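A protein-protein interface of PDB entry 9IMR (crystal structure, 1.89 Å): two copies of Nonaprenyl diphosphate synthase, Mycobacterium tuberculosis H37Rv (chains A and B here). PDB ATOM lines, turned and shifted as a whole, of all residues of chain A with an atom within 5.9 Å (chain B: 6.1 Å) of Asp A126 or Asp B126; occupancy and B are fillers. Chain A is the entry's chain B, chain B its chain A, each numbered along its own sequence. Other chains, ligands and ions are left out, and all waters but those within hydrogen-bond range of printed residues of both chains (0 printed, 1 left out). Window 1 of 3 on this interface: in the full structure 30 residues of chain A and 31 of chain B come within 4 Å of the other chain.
Of the 15 printed residues of chain B, 7 touch a printed residue of chain A. Of the 15 printed residues of chain A, 8 touch a printed residue of chain B. Hydrophobic or aromatic side chains of chain A within 4 Å of the printed part of chain B: His A96, Ile A122, Tyr A127, Ala A130, Phe A151 and Val A155.
The side-chain carboxylate (OD2) of Asp A126 lies within hydrogen-bond range of a ring nitrogen (ND1) of His B96, at 2.6 Å. OD2 of Asp B126 lies within hydrogen-bond range of ND1 of His A96 (2.5 Å).
NE2 of His B96 lies within hydrogen-bond range of O of Ile B122 (2.8 Å). The side-chain carboxylate (OD1) of Asp B126 sits close to a ring nitrogen (NE2) of His B96 (3.3 Å). The backbone carbonyl oxygen (O) of Tyr B127 sits at hydrogen-bond distance from the side-chain hydroxyl (OG1) of Thr B131, 3.3 Å away. The backbone carbonyl oxygen of Ile A122 is in hydrogen-bond range of a ring nitrogen (NE2) of His A96 (2.8 Å). A ring nitrogen (NE2) of His A96 lies close to the side-chain carboxylate (OD1) of Asp A126 (3.3 Å). O of Tyr A127 is in hydrogen-bond range of OG1 of Thr A131 (3.0 Å).
His A96 touches Ile B122, and with the chains exchanged Ile A122 touches His B96. Asp A126 touches Phe B151, and with the chains exchanged Phe A151 touches Asp B126. Asp A126 touches Val B155, and with the chains exchanged Val A155 touches Asp B126. Ala A130 touches Phe B151, but with the chains exchanged Phe A151 does not touch Ala B130 (4.01 Å). Positions printed for both chains: 92, 96, 121, 122, 123, 124, 125, 126, 127, 128, 129, 130, 131, 151 and 155.
Among the printed residues, merely in contact across the chains: His A96 with His B96 (3.8 Å), His A96 with Ile B122 (3.9 Å), Ile A122 with His B96 (3.6 Å), Leu A123 with Val B155 (3.2 Å), Asp A126 with Asp B126 (3.6 Å), Asp A126 with Phe B151 (3.5 Å), Asp A126 with Val B155 (3.8 Å), Tyr A127 with Val B155 (3.8 Å), Ala A130 with Phe B151 (3.9 Å), Phe A151 with Asp B126 (3.5 Å), Val A155 with Leu B123 (3.3 Å), Val A155 with Asp B126 (3.9 Å) and Val A155 with Tyr B127 (3.8 Å).
Of the printed residues of chain B, Asp A126 touches His B96 (2.6 Å), Asp B126 (3.6 Å), Phe B151 (3.5 Å) and Val B155 (3.8 Å). Of the printed residues of chain A, Leu B123 touches Val A155. Of chain A, only His A96 (2.5 Å), Asp A126 (3.6 Å), Phe A151 (3.5 Å) and Val A155 (3.9 Å) come within 4 Å of Asp B126. Printed residues of chain A within 4 Å of Tyr B127: Val A155 (3.8 Å). Of the printed residues of chain A, Val B155 touches Leu A123 (3.2 Å), Asp A126 (3.8 Å) and Tyr A127 (3.8 Å).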
ATOM      1  N   ALA A  92      21.764  18.087  10.387  1.00  0.00           N
ATOM      2  CA  ALA A  92      21.305  18.819   9.180  1.00  0.00           C
ATOM      3  C   ALA A  92      20.265  19.893   9.543  1.00  0.00           C
ATOM      4  O   ALA A  92      20.378  21.056   9.078  1.00  0.00           O
ATOM      5  CB  ALA A  92      20.749  17.857   8.170  1.00  0.00           C
ATOM      6  N   HIS A  96      20.110  24.218   9.165  1.00  0.00           N
ATOM      7  CA  HIS A  96      19.054  25.019   8.493  1.00  0.00           C
ATOM      8  C   HIS A  96      18.338  25.896   9.533  1.00  0.00           C
ATOM      9  O   HIS A  96      18.010  27.071   9.230  1.00  0.00           O
ATOM     10  CB  HIS A  96      18.118  24.149   7.668  1.00  0.00           C
ATOM     11  CG  HIS A  96      18.782  23.623   6.441  1.00  0.00           C
ATOM     12  ND1 HIS A  96      18.110  22.882   5.500  1.00  0.00           N
ATOM     13  CD2 HIS A  96      20.071  23.733   6.024  1.00  0.00           C
ATOM     14  CE1 HIS A  96      18.965  22.556   4.550  1.00  0.00           C
ATOM     15  NE2 HIS A  96      20.164  23.097   4.825  1.00  0.00           N
ATOM     16  N   ALA A 121      26.252  27.255   5.457  1.00  0.00           N
ATOM     17  CA  ALA A 121      25.374  26.573   6.431  1.00  0.00           C
ATOM     18  C   ALA A 121      24.256  25.824   5.696  1.00  0.00           C
ATOM     19  O   ALA A 121      24.047  24.638   6.065  1.00  0.00           O
ATOM     20  CB  ALA A 121      24.852  27.536   7.467  1.00  0.00           C
ATOM     21  N   ILE A 122      23.565  26.453   4.733  1.00  0.00           N
ATOM     22  CA  ILE A 122      22.488  25.787   3.932  1.00  0.00           C
ATOM     23  C   ILE A 122      23.094  24.554   3.256  1.00  0.00           C
ATOM     24  O   ILE A 122      22.499  23.466   3.349  1.00  0.00           O
ATOM     25  CB  ILE A 122      21.838  26.762   2.918  1.00  0.00           C
ATOM     26  CG1 ILE A 122      21.021  27.841   3.628  1.00  0.00           C
ATOM     27  CG2 ILE A 122      20.990  26.017   1.910  1.00  0.00           C
ATOM     28  CD1 ILE A 122      20.734  29.003   2.749  1.00  0.00           C
ATOM     29  N   LEU A 123      24.233  24.703   2.597  1.00  0.00           N
ATOM     30  CA  LEU A 123      24.843  23.571   1.837  1.00  0.00           C
ATOM     31  C   LEU A 123      25.370  22.472   2.771  1.00  0.00           C
ATOM     32  O   LEU A 123      25.233  21.309   2.396  1.00  0.00           O
ATOM     33  CB  LEU A 123      25.933  24.150   0.951  1.00  0.00           C
ATOM     34  CG  LEU A 123      25.373  25.030  -0.164  1.00  0.00           C
ATOM     35  CD1 LEU A 123      26.487  25.698  -0.908  1.00  0.00           C
ATOM     36  CD2 LEU A 123      24.516  24.203  -1.108  1.00  0.00           C
ATOM     37  N   ALA A 124      25.931  22.820   3.920  1.00  0.00           N
ATOM     38  CA  ALA A 124      26.402  21.830   4.907  1.00  0.00           C
ATOM     39  C   ALA A 124      25.189  20.974   5.300  1.00  0.00           C
ATOM     40  O   ALA A 124      25.291  19.729   5.276  1.00  0.00           O
ATOM     41  CB  ALA A 124      27.068  22.491   6.102  1.00  0.00           C
ATOM     42  N   GLY A 125      24.066  21.605   5.616  1.00  0.00           N
ATOM     43  CA  GLY A 125      22.811  20.895   5.957  1.00  0.00           C
ATOM     44  C   GLY A 125      22.336  19.992   4.824  1.00  0.00           C
ATOM     45  O   GLY A 125      21.947  18.825   5.079  1.00  0.00           O
ATOM     46  N   ASP A 126      22.413  20.467   3.584  1.00  0.00           N
ATOM     47  CA  ASP A 126      21.979  19.661   2.414  1.00  0.00           C
ATOM     48  C   ASP A 126      22.936  18.467   2.284  1.00  0.00           C
ATOM     49  O   ASP A 126      22.462  17.367   1.968  1.00  0.00           O
ATOM     50  CB  ASP A 126      21.962  20.508   1.150  1.00  0.00           C
ATOM     51  CG  ASP A 126      20.850  21.535   1.094  1.00  0.00           C
ATOM     52  OD1 ASP A 126      19.925  21.462   1.953  1.00  0.00           O
ATOM     53  OD2 ASP A 126      20.897  22.387   0.144  1.00  0.00           O
ATOM     54  N   TYR A 127      24.232  18.668   2.477  1.00  0.00           N
ATOM     55  CA  TYR A 127      25.204  17.552   2.348  1.00  0.00           C
ATOM     56  C   TYR A 127      24.882  16.489   3.409  1.00  0.00           C
ATOM     57  O   TYR A 127      24.920  15.275   3.139  1.00  0.00           O
ATOM     58  CB  TYR A 127      26.636  18.058   2.476  1.00  0.00           C
ATOM     59  CG  TYR A 127      27.628  16.979   2.197  1.00  0.00           C
ATOM     60  CD1 TYR A 127      28.059  16.173   3.226  1.00  0.00           C
ATOM     61  CD2 TYR A 127      28.091  16.724   0.919  1.00  0.00           C
ATOM     62  CE1 TYR A 127      28.919  15.116   3.000  1.00  0.00           C
ATOM     63  CE2 TYR A 127      28.997  15.698   0.677  1.00  0.00           C
ATOM     64  CZ  TYR A 127      29.409  14.903   1.729  1.00  0.00           C
ATOM     65  OH  TYR A 127      30.288  13.877   1.587  1.00  0.00           O
ATOM     66  N   LEU A 128      24.600  16.917   4.635  1.00  0.00           N
ATOM     67  CA  LEU A 128      24.268  15.960   5.733  1.00  0.00           C
ATOM     68  C   LEU A 128      23.021  15.151   5.365  1.00  0.00           C
ATOM     69  O   LEU A 128      22.972  13.923   5.642  1.00  0.00           O
ATOM     70  CB  LEU A 128      24.130  16.759   7.021  1.00  0.00           C
ATOM     71  CG  LEU A 128      25.463  17.258   7.578  1.00  0.00           C
ATOM     72  CD1 LEU A 128      25.254  18.321   8.648  1.00  0.00           C
ATOM     73  CD2 LEU A 128      26.272  16.114   8.170  1.00  0.00           C
ATOM     74  N   LEU A 129      22.038  15.768   4.728  1.00  0.00           N
ATOM     75  CA  LEU A 129      20.816  15.039   4.309  1.00  0.00           C
ATOM     76  C   LEU A 129      21.207  14.012   3.239  1.00  0.00           C
ATOM     77  O   LEU A 129      20.707  12.884   3.323  1.00  0.00           O
ATOM     78  CB  LEU A 129      19.748  16.010   3.819  1.00  0.00           C
ATOM     79  CG  LEU A 129      19.261  16.998   4.871  1.00  0.00           C
ATOM     80  CD1 LEU A 129      18.389  18.099   4.257  1.00  0.00           C
ATOM     81  CD2 LEU A 129      18.549  16.266   5.999  1.00  0.00           C
ATOM     82  N   ALA A 130      22.084  14.345   2.281  1.00  0.00           N
ATOM     83  CA  ALA A 130      22.579  13.351   1.290  1.00  0.00           C
ATOM     84  C   ALA A 130      23.265  12.185   2.009  1.00  0.00           C
ATOM     85  O   ALA A 130      23.033  11.012   1.636  1.00  0.00           O
ATOM     86  CB  ALA A 130      23.530  13.986   0.304  1.00  0.00           C
ATOM     87  N   THR A 131      24.052  12.506   3.021  1.00  0.00           N
ATOM     88  CA  THR A 131      24.859  11.534   3.794  1.00  0.00           C
ATOM     89  C   THR A 131      23.917  10.598   4.553  1.00  0.00           C
ATOM     90  O   THR A 131      24.140   9.339   4.530  1.00  0.00           O
ATOM     91  CB  THR A 131      25.858  12.271   4.697  1.00  0.00           C
ATOM     92  OG1 THR A 131      26.704  13.023   3.813  1.00  0.00           O
ATOM     93  CG2 THR A 131      26.703  11.322   5.529  1.00  0.00           C
ATOM     94  N   PHE A 151      11.438  12.822   7.687  1.00  0.00           N
ATOM     95  CA  PHE A 151      11.982  14.133   7.297  1.00  0.00           C
ATOM     96  C   PHE A 151      10.876  15.007   6.707  1.00  0.00           C
ATOM     97  O   PHE A 151      10.899  16.164   7.017  1.00  0.00           O
ATOM     98  CB  PHE A 151      13.189  13.963   6.389  1.00  0.00           C
ATOM     99  CG  PHE A 151      13.938  15.258   6.252  1.00  0.00           C
ATOM    100  CD1 PHE A 151      14.478  15.890   7.364  1.00  0.00           C
ATOM    101  CD2 PHE A 151      13.999  15.887   5.021  1.00  0.00           C
ATOM    102  CE1 PHE A 151      15.130  17.113   7.237  1.00  0.00           C
ATOM    103  CE2 PHE A 151      14.690  17.090   4.886  1.00  0.00           C
ATOM    104  CZ  PHE A 151      15.204  17.725   6.001  1.00  0.00           C
ATOM    105  N   VAL A 155       9.961  18.656   8.381  1.00  0.00           N
ATOM    106  CA  VAL A 155       9.919  19.897   7.573  1.00  0.00           C
ATOM    107  C   VAL A 155       8.514  20.503   7.616  1.00  0.00           C
ATOM    108  O   VAL A 155       8.411  21.735   7.638  1.00  0.00           O
ATOM    109  CB  VAL A 155      10.433  19.621   6.151  1.00  0.00           C
ATOM    110  CG1 VAL A 155      10.241  20.816   5.240  1.00  0.00           C
ATOM    111  CG2 VAL A 155      11.895  19.233   6.214  1.00  0.00           C
ATOM    112  N   ALA B  92      14.384  21.145  -5.956  1.00  0.00           N
ATOM    113  CA  ALA B  92      14.928  21.407  -4.607  1.00  0.00           C
ATOM    114  C   ALA B  92      16.145  22.345  -4.682  1.00  0.00           C
ATOM    115  O   ALA B  92      16.255  23.279  -3.848  1.00  0.00           O
ATOM    116  CB  ALA B  92      15.270  20.122  -3.936  1.00  0.00           C
ATOM    117  N   HIS B  96      16.979  26.360  -2.935  1.00  0.00           N
ATOM    118  CA  HIS B  96      18.181  26.729  -2.123  1.00  0.00           C
ATOM    119  C   HIS B  96      19.059  27.712  -2.900  1.00  0.00           C
ATOM    120  O   HIS B  96      19.619  28.650  -2.289  1.00  0.00           O
ATOM    121  CB  HIS B  96      18.914  25.482  -1.632  1.00  0.00           C
ATOM    122  CG  HIS B  96      18.158  24.812  -0.552  1.00  0.00           C
ATOM    123  ND1 HIS B  96      18.694  23.765   0.195  1.00  0.00           N
ATOM    124  CD2 HIS B  96      16.913  25.077  -0.070  1.00  0.00           C
ATOM    125  CE1 HIS B  96      17.782  23.418   1.077  1.00  0.00           C
ATOM    126  NE2 HIS B  96      16.677  24.194   0.929  1.00  0.00           N
ATOM    127  N   ALA B 121      11.423  29.165   1.639  1.00  0.00           N
ATOM    128  CA  ALA B 121      12.143  28.619   0.468  1.00  0.00           C
ATOM    129  C   ALA B 121      13.091  27.523   0.921  1.00  0.00           C
ATOM    130  O   ALA B 121      13.163  26.508   0.232  1.00  0.00           O
ATOM    131  CB  ALA B 121      12.848  29.743  -0.265  1.00  0.00           C
ATOM    132  N   ILE B 122      13.836  27.732   2.021  1.00  0.00           N
ATOM    133  CA  ILE B 122      14.751  26.720   2.580  1.00  0.00           C
ATOM    134  C   ILE B 122      13.921  25.454   2.842  1.00  0.00           C
ATOM    135  O   ILE B 122      14.331  24.350   2.440  1.00  0.00           O
ATOM    136  CB  ILE B 122      15.513  27.275   3.804  1.00  0.00           C
ATOM    137  CG1 ILE B 122      16.476  28.388   3.372  1.00  0.00           C
ATOM    138  CG2 ILE B 122      16.267  26.145   4.501  1.00  0.00           C
ATOM    139  CD1 ILE B 122      17.140  29.110   4.547  1.00  0.00           C
ATOM    140  N   LEU B 123      12.774  25.596   3.493  1.00  0.00           N
ATOM    141  CA  LEU B 123      11.992  24.419   3.937  1.00  0.00           C
ATOM    142  C   LEU B 123      11.316  23.760   2.734  1.00  0.00           C
ATOM    143  O   LEU B 123      11.292  22.515   2.663  1.00  0.00           O
ATOM    144  CB  LEU B 123      10.963  24.913   4.948  1.00  0.00           C
ATOM    145  CG  LEU B 123      11.548  25.302   6.296  1.00  0.00           C
ATOM    146  CD1 LEU B 123      10.487  25.894   7.161  1.00  0.00           C
ATOM    147  CD2 LEU B 123      12.217  24.139   7.015  1.00  0.00           C
ATOM    148  N   ALA B 124      10.878  24.530   1.757  1.00  0.00           N
ATOM    149  CA  ALA B 124      10.294  23.946   0.538  1.00  0.00           C
ATOM    150  C   ALA B 124      11.376  23.108  -0.153  1.00  0.00           C
ATOM    151  O   ALA B 124      11.077  21.985  -0.548  1.00  0.00           O
ATOM    152  CB  ALA B 124       9.704  25.000  -0.359  1.00  0.00           C
ATOM    153  N   GLY B 125      12.625  23.590  -0.199  1.00  0.00           N
ATOM    154  CA  GLY B 125      13.748  22.830  -0.790  1.00  0.00           C
ATOM    155  C   GLY B 125      14.003  21.538  -0.016  1.00  0.00           C
ATOM    156  O   GLY B 125      14.175  20.471  -0.648  1.00  0.00           O
ATOM    157  N   ASP B 126      14.015  21.616   1.320  1.00  0.00           N
ATOM    158  CA  ASP B 126      14.225  20.443   2.196  1.00  0.00           C
ATOM    159  C   ASP B 126      13.116  19.420   1.961  1.00  0.00           C
ATOM    160  O   ASP B 126      13.437  18.211   1.858  1.00  0.00           O
ATOM    161  CB  ASP B 126      14.339  20.833   3.658  1.00  0.00           C
ATOM    162  CG  ASP B 126      15.622  21.560   4.003  1.00  0.00           C
ATOM    163  OD1 ASP B 126      16.494  21.674   3.097  1.00  0.00           O
ATOM    164  OD2 ASP B 126      15.803  21.941   5.189  1.00  0.00           O
ATOM    165  N   TYR B 127      11.872  19.862   1.866  1.00  0.00           N
ATOM    166  CA  TYR B 127      10.717  18.959   1.667  1.00  0.00           C
ATOM    167  C   TYR B 127      10.882  18.172   0.349  1.00  0.00           C
ATOM    168  O   TYR B 127      10.624  16.947   0.352  1.00  0.00           O
ATOM    169  CB  TYR B 127       9.403  19.734   1.652  1.00  0.00           C
ATOM    170  CG  TYR B 127       8.235  18.799   1.805  1.00  0.00           C
ATOM    171  CD1 TYR B 127       7.731  18.139   0.697  1.00  0.00           C
ATOM    172  CD2 TYR B 127       7.670  18.521   3.045  1.00  0.00           C
ATOM    173  CE1 TYR B 127       6.662  17.263   0.797  1.00  0.00           C
ATOM    174  CE2 TYR B 127       6.638  17.614   3.160  1.00  0.00           C
ATOM    175  CZ  TYR B 127       6.121  17.002   2.034  1.00  0.00           C
ATOM    176  OH  TYR B 127       5.084  16.145   2.092  1.00  0.00           O
ATOM    177  N   LEU B 128      11.234  18.858  -0.727  1.00  0.00           N
ATOM    178  CA  LEU B 128      11.401  18.267  -2.086  1.00  0.00           C
ATOM    179  C   LEU B 128      12.451  17.147  -2.055  1.00  0.00           C
ATOM    180  O   LEU B 128      12.312  16.162  -2.780  1.00  0.00           O
ATOM    181  CB  LEU B 128      11.752  19.389  -3.064  1.00  0.00           C
ATOM    182  CG  LEU B 128      10.590  20.271  -3.474  1.00  0.00           C
ATOM    183  CD1 LEU B 128      11.052  21.519  -4.180  1.00  0.00           C
ATOM    184  CD2 LEU B 128       9.600  19.534  -4.356  1.00  0.00           C
ATOM    185  N   LEU B 129      13.456  17.272  -1.204  1.00  0.00           N
ATOM    186  CA  LEU B 129      14.471  16.223  -1.020  1.00  0.00           C
ATOM    187  C   LEU B 129      13.805  15.001  -0.429  1.00  0.00           C
ATOM    188  O   LEU B 129      14.110  13.909  -0.890  1.00  0.00           O
ATOM    189  CB  LEU B 129      15.601  16.706  -0.110  1.00  0.00           C
ATOM    190  CG  LEU B 129      16.460  17.831  -0.670  1.00  0.00           C
ATOM    191  CD1 LEU B 129      17.601  18.086   0.322  1.00  0.00           C
ATOM    192  CD2 LEU B 129      16.999  17.472  -2.061  1.00  0.00           C
ATOM    193  N   ALA B 130      12.893  15.174   0.532  1.00  0.00           N
ATOM    194  CA  ALA B 130      12.173  14.049   1.163  1.00  0.00           C
ATOM    195  C   ALA B 130      11.292  13.378   0.114  1.00  0.00           C
ATOM    196  O   ALA B 130      11.214  12.135   0.095  1.00  0.00           O
ATOM    197  CB  ALA B 130      11.351  14.533   2.338  1.00  0.00           C
ATOM    198  N   THR B 131      10.636  14.185  -0.714  1.00  0.00           N
ATOM    199  CA  THR B 131       9.753  13.708  -1.807  1.00  0.00           C
ATOM    200  C   THR B 131      10.588  12.864  -2.778  1.00  0.00           C
ATOM    201  O   THR B 131      10.157  11.749  -3.145  1.00  0.00           O
ATOM    202  CB  THR B 131       9.057  14.884  -2.486  1.00  0.00           C
ATOM    203  OG1 THR B 131       8.309  15.565  -1.478  1.00  0.00           O
ATOM    204  CG2 THR B 131       8.123  14.450  -3.590  1.00  0.00           C
ATOM    205  N   PHE B 151      23.194  13.948  -5.378  1.00  0.00           N
ATOM    206  CA  PHE B 151      22.899  15.145  -4.563  1.00  0.00           C
ATOM    207  C   PHE B 151      24.144  15.572  -3.765  1.00  0.00           C
ATOM    208  O   PHE B 151      24.448  16.791  -3.688  1.00  0.00           O
ATOM    209  CB  PHE B 151      21.666  14.922  -3.706  1.00  0.00           C
ATOM    210  CG  PHE B 151      21.221  16.206  -3.058  1.00  0.00           C
ATOM    211  CD1 PHE B 151      20.911  17.309  -3.839  1.00  0.00           C
ATOM    212  CD2 PHE B 151      21.185  16.335  -1.685  1.00  0.00           C
ATOM    213  CE1 PHE B 151      20.484  18.484  -3.242  1.00  0.00           C
ATOM    214  CE2 PHE B 151      20.745  17.513  -1.092  1.00  0.00           C
ATOM    215  CZ  PHE B 151      20.401  18.585  -1.875  1.00  0.00           C
ATOM    216  N   VAL B 155      25.802  19.306  -4.305  1.00  0.00           N
ATOM    217  CA  VAL B 155      25.994  20.166  -3.107  1.00  0.00           C
ATOM    218  C   VAL B 155      27.468  20.522  -2.961  1.00  0.00           C
ATOM    219  O   VAL B 155      27.761  21.702  -2.666  1.00  0.00           O
ATOM    220  CB  VAL B 155      25.403  19.506  -1.844  1.00  0.00           C
ATOM    221  CG1 VAL B 155      25.822  20.292  -0.605  1.00  0.00           C
ATOM    222  CG2 VAL B 155      23.888  19.397  -1.956  1.00  0.00           C
